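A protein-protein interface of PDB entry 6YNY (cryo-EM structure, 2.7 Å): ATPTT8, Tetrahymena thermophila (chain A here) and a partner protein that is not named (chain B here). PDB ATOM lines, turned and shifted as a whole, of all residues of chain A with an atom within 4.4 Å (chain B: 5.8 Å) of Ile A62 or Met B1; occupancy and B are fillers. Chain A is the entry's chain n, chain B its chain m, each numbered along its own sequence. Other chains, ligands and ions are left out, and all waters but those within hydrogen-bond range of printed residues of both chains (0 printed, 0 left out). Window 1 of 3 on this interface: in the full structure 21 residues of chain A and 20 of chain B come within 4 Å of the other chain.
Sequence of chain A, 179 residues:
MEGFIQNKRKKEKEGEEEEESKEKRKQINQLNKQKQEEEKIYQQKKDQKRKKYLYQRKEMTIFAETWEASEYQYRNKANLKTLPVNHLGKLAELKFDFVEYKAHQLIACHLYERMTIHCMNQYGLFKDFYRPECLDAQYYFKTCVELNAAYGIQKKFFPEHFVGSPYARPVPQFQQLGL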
ATOM      1  N   THR A  61     -28.053  21.290  10.206  1.00  0.00           N
ATOM      2  CA  THR A  61     -27.799  21.569   8.799  1.00  0.00           C
ATOM      3  C   THR A  61     -26.818  22.721   8.650  1.00  0.00           C
ATOM      4  O   THR A  61     -26.826  23.663   9.441  1.00  0.00           O
ATOM      5  CB  THR A  61     -29.097  21.911   8.049  1.00  0.00           C
ATOM      6  OG1 THR A  61     -30.020  20.824   8.160  1.00  0.00           O
ATOM      7  CG2 THR A  61     -28.818  22.173   6.584  1.00  0.00           C
ATOM      8  N   ILE A  62     -25.968  22.637   7.633  1.00  0.00           N
ATOM      9  CA  ILE A  62     -25.012  23.693   7.326  1.00  0.00           C
ATOM     10  C   ILE A  62     -25.657  24.630   6.315  1.00  0.00           C
ATOM     11  O   ILE A  62     -26.090  24.197   5.242  1.00  0.00           O
ATOM     12  CB  ILE A  62     -23.698  23.118   6.784  1.00  0.00           C
ATOM     13  CG1 ILE A  62     -23.119  22.105   7.769  1.00  0.00           C
ATOM     14  CG2 ILE A  62     -22.696  24.227   6.548  1.00  0.00           C
ATOM     15  CD1 ILE A  62     -21.881  21.417   7.271  1.00  0.00           C
ATOM     16  N   PHE A  63     -25.722  25.910   6.658  1.00  0.00           N
ATOM     17  CA  PHE A  63     -26.329  26.934   5.819  1.00  0.00           C
ATOM     18  C   PHE A  63     -25.273  27.808   5.153  1.00  0.00           C
ATOM     19  O   PHE A  63     -25.431  29.023   5.033  1.00  0.00           O
ATOM     20  CB  PHE A  63     -27.301  27.780   6.632  1.00  0.00           C
ATOM     21  CG  PHE A  63     -28.455  26.998   7.183  1.00  0.00           C
ATOM     22  CD1 PHE A  63     -29.472  26.570   6.352  1.00  0.00           C
ATOM     23  CD2 PHE A  63     -28.525  26.687   8.525  1.00  0.00           C
ATOM     24  CE1 PHE A  63     -30.531  25.851   6.848  1.00  0.00           C
ATOM     25  CE2 PHE A  63     -29.589  25.965   9.023  1.00  0.00           C
ATOM     26  CZ  PHE A  63     -30.589  25.549   8.183  1.00  0.00           C
ATOM     27  N   ALA A  64     -24.175  27.196   4.726  1.00  0.00           N
ATOM     28  CA  ALA A  64     -23.102  27.916   4.059  1.00  0.00           C
ATOM     29  C   ALA A  64     -22.293  26.923   3.238  1.00  0.00           C
ATOM     30  O   ALA A  64     -22.561  25.719   3.241  1.00  0.00           O
ATOM     31  CB  ALA A  64     -22.221  28.649   5.070  1.00  0.00           C
ATOM     32  N   TRP A  67     -17.352  25.491   6.576  1.00  0.00           N
ATOM     33  CA  TRP A  67     -17.551  25.208   7.985  1.00  0.00           C
ATOM     34  C   TRP A  67     -16.195  25.074   8.654  1.00  0.00           C
ATOM     35  O   TRP A  67     -15.252  24.542   8.064  1.00  0.00           O
ATOM     36  CB  TRP A  67     -18.367  23.932   8.189  1.00  0.00           C
ATOM     37  CG  TRP A  67     -17.784  22.738   7.516  1.00  0.00           C
ATOM     38  CD1 TRP A  67     -16.974  21.801   8.074  1.00  0.00           C
ATOM     39  CD2 TRP A  67     -17.963  22.351   6.150  1.00  0.00           C
ATOM     40  NE1 TRP A  67     -16.636  20.852   7.146  1.00  0.00           N
ATOM     41  CE2 TRP A  67     -17.230  21.168   5.954  1.00  0.00           C
ATOM     42  CE3 TRP A  67     -18.671  22.891   5.075  1.00  0.00           C
ATOM     43  CZ2 TRP A  67     -17.185  20.516   4.730  1.00  0.00           C
ATOM     44  CZ3 TRP A  67     -18.624  22.241   3.862  1.00  0.00           C
ATOM     45  CH2 TRP A  67     -17.887  21.067   3.698  1.00  0.00           C
ATOM     46  N   TYR A  72     -16.498  20.527  14.132  1.00  0.00           N
ATOM     47  CA  TYR A  72     -16.998  19.168  13.967  1.00  0.00           C
ATOM     48  C   TYR A  72     -16.004  18.136  14.483  1.00  0.00           C
ATOM     49  O   TYR A  72     -16.069  16.965  14.100  1.00  0.00           O
ATOM     50  CB  TYR A  72     -17.351  18.911  12.503  1.00  0.00           C
ATOM     51  CG  TYR A  72     -18.532  19.730  12.049  1.00  0.00           C
ATOM     52  CD1 TYR A  72     -18.361  20.998  11.520  1.00  0.00           C
ATOM     53  CD2 TYR A  72     -19.821  19.244  12.173  1.00  0.00           C
ATOM     54  CE1 TYR A  72     -19.439  21.750  11.119  1.00  0.00           C
ATOM     55  CE2 TYR A  72     -20.903  19.990  11.772  1.00  0.00           C
ATOM     56  CZ  TYR A  72     -20.706  21.242  11.248  1.00  0.00           C
ATOM     57  OH  TYR A  72     -21.788  21.987  10.850  1.00  0.00           O
ATOM     58  N   ALA A 108     -21.556  21.067   0.606  1.00  0.00           N
ATOM     59  CA  ALA A 108     -21.202  19.719   1.022  1.00  0.00           C
ATOM     60  C   ALA A 108     -21.907  18.669   0.176  1.00  0.00           C
ATOM     61  O   ALA A 108     -23.122  18.731  -0.027  1.00  0.00           O
ATOM     62  CB  ALA A 108     -21.551  19.520   2.493  1.00  0.00           C
ATOM     63  N   ASN A 148     -22.549  13.253   6.868  1.00  0.00           N
ATOM     64  CA  ASN A 148     -23.115  14.562   7.166  1.00  0.00           C
ATOM     65  C   ASN A 148     -24.466  14.446   7.854  1.00  0.00           C
ATOM     66  O   ASN A 148     -24.808  15.285   8.693  1.00  0.00           O
ATOM     67  CB  ASN A 148     -23.225  15.382   5.886  1.00  0.00           C
ATOM     68  CG  ASN A 148     -21.952  16.130   5.568  1.00  0.00           C
ATOM     69  OD1 ASN A 148     -21.749  17.254   6.022  1.00  0.00           O
ATOM     70  ND2 ASN A 148     -21.082  15.507   4.794  1.00  0.00           N
ATOM     71  N   ALA A 149     -25.246  13.421   7.516  1.00  0.00           N
ATOM     72  CA  ALA A 149     -26.495  13.189   8.230  1.00  0.00           C
ATOM     73  C   ALA A 149     -26.234  12.786   9.673  1.00  0.00           C
ATOM     74  O   ALA A 149     -26.981  13.173  10.578  1.00  0.00           O
ATOM     75  CB  ALA A 149     -27.315  12.116   7.521  1.00  0.00           C
ATOM     76  N   GLY A 152     -24.756  15.875  11.448  1.00  0.00           N
ATOM     77  CA  GLY A 152     -25.809  16.856  11.632  1.00  0.00           C
ATOM     78  C   GLY A 152     -26.728  16.510  12.786  1.00  0.00           C
ATOM     79  O   GLY A 152     -27.123  17.383  13.561  1.00  0.00           O
ATOM     80  N   MET B   1     -24.279  18.471   8.352  1.00  0.00           N
ATOM     81  CA  MET B   1     -25.153  18.823   7.197  1.00  0.00           C
ATOM     82  C   MET B   1     -26.241  17.778   6.985  1.00  0.00           C
ATOM     83  O   MET B   1     -26.193  16.995   6.037  1.00  0.00           O
ATOM     84  CB  MET B   1     -24.318  18.972   5.929  1.00  0.00           C
ATOM     85  CG  MET B   1     -25.091  19.388   4.698  1.00  0.00           C
ATOM     86  SD  MET B   1     -25.811  21.025   4.828  1.00  0.00           S
ATOM     87  CE  MET B   1     -26.245  21.282   3.119  1.00  0.00           C
ATOM     88  N   ASP B   2     -27.223  17.770   7.877  1.00  0.00           N
ATOM     89  CA  ASP B   2     -28.365  16.883   7.752  1.00  0.00           C
ATOM     90  C   ASP B   2     -29.433  17.522   6.869  1.00  0.00           C
ATOM     91  O   ASP B   2     -29.380  18.709   6.541  1.00  0.00           O
ATOM     92  CB  ASP B   2     -28.931  16.541   9.130  1.00  0.00           C
ATOM     93  CG  ASP B   2     -29.271  17.772   9.940  1.00  0.00           C
ATOM     94  OD1 ASP B   2     -28.587  18.801   9.766  1.00  0.00           O
ATOM     95  OD2 ASP B   2     -30.219  17.710  10.750  1.00  0.00           O
ATOM     96  N   ASN B   3     -30.415  16.714   6.483  1.00  0.00           N
ATOM     97  CA  ASN B   3     -31.456  17.142   5.554  1.00  0.00           C
ATOM     98  C   ASN B   3     -30.834  17.677   4.267  1.00  0.00           C
ATOM     99  O   ASN B   3     -31.191  18.744   3.767  1.00  0.00           O
ATOM    100  CB  ASN B   3     -32.369  18.185   6.197  1.00  0.00           C
ATOM    101  CG  ASN B   3     -33.090  17.656   7.412  1.00  0.00           C
ATOM    102  OD1 ASN B   3     -34.047  16.893   7.297  1.00  0.00           O
ATOM    103  ND2 ASN B   3     -32.644  18.070   8.586  1.00  0.00           N
ATOM    104  N   TYR B   4     -29.882  16.914   3.732  1.00  0.00           N
ATOM    105  CA  TYR B   4     -29.163  17.344   2.539  1.00  0.00           C
ATOM    106  C   TYR B   4     -30.104  17.489   1.350  1.00  0.00           C
ATOM    107  O   TYR B   4     -30.229  18.569   0.765  1.00  0.00           O
ATOM    108  CB  TYR B   4     -28.044  16.354   2.223  1.00  0.00           C
ATOM    109  CG  TYR B   4     -27.444  16.536   0.852  1.00  0.00           C
ATOM    110  CD1 TYR B   4     -26.418  17.437   0.636  1.00  0.00           C
ATOM    111  CD2 TYR B   4     -27.909  15.807  -0.228  1.00  0.00           C
ATOM    112  CE1 TYR B   4     -25.875  17.606  -0.611  1.00  0.00           C
ATOM    113  CE2 TYR B   4     -27.373  15.972  -1.476  1.00  0.00           C
ATOM    114  CZ  TYR B   4     -26.357  16.870  -1.665  1.00  0.00           C
ATOM    115  OH  TYR B   4     -25.825  17.030  -2.917  1.00  0.00           O
ATOM    116  N   ALA B   7     -32.597  20.338   1.645  1.00  0.00           N
ATOM    117  CA  ALA B   7     -32.027  21.666   1.465  1.00  0.00           C
ATOM    118  C   ALA B   7     -31.645  21.908   0.012  1.00  0.00           C
ATOM    119  O   ALA B   7     -31.934  22.970  -0.548  1.00  0.00           O
ATOM    120  CB  ALA B   7     -30.815  21.835   2.376  1.00  0.00           C
ATOM    121  N   ILE B   8     -30.992  20.930  -0.617  1.00  0.00           N
ATOM    122  CA  ILE B   8     -30.609  21.073  -2.016  1.00  0.00           C
ATOM    123  C   ILE B   8     -31.832  21.300  -2.889  1.00  0.00           C
ATOM    124  O   ILE B   8     -31.751  21.972  -3.924  1.00  0.00           O
ATOM    125  CB  ILE B   8     -29.811  19.837  -2.471  1.00  0.00           C
ATOM    126  CG1 ILE B   8     -28.492  19.736  -1.703  1.00  0.00           C
ATOM    127  CG2 ILE B   8     -29.548  19.876  -3.950  1.00  0.00           C
ATOM    128  CD1 ILE B   8     -27.564  20.905  -1.891  1.00  0.00           C
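The side-chain sulfur (SD) of Met B1 sits at hydrogen-bond distance from the backbone NH (N) of Ile A62 (3.2 Å).
N of Met B1 lies within hydrogen-bond range of O of Asn A148 (3.2 Å).
The backbone NH (N) of Thr A61 sits at hydrogen-bond distance from the side-chain carboxylate (OD1) of Asp B2.
The side-chain carboxylate (OD2) of Asp B2 sits at hydrogen-bond distance from the side-chain amide nitrogen (ND2) of Asn B3 (3.3 Å).
Among the printed residues, merely in contact across the chains: Ala A108 with Tyr B4, Asn A148 with Asp B2, Thr A61 with Met B1, Thr A61 with Asn B3, Gly A152 with Asp B2, Gly A152 with Met B1 and Ala A149 with Met B1.
Of chain B, only Met B1 comes within 4 Å of Ile A62.
Of the printed residues of chain A, Met B1 touches Thr A61, Ile A62, Asn A148, Ala A149 and Gly A152.
Of the printed residues of chain B, Ala A108 touches Tyr B4.
Printed residues of chain A within 4 Å of Asn B3: Thr A61 (3.8 Å).
Ile B8 touches none of the printed residues of chain A.
The nearest printed residue of chain A that does not touch Met B1 is Ala A108 (4.2 Å).
The nearest printed residue of chain B that does not touch Ala A108 is Met B1 (4.2 Å).
Hydrophobic or aromatic side chains of chain B within 4 Å of the printed part of chain A: Met B1 and Tyr B4.
Along chain B the printed residues that touch a printed residue of chain A span positions 1 to 4.
Hydrophobic or aromatic side chains of chain A within 4 Å of the printed part of chain B: Ile A62.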
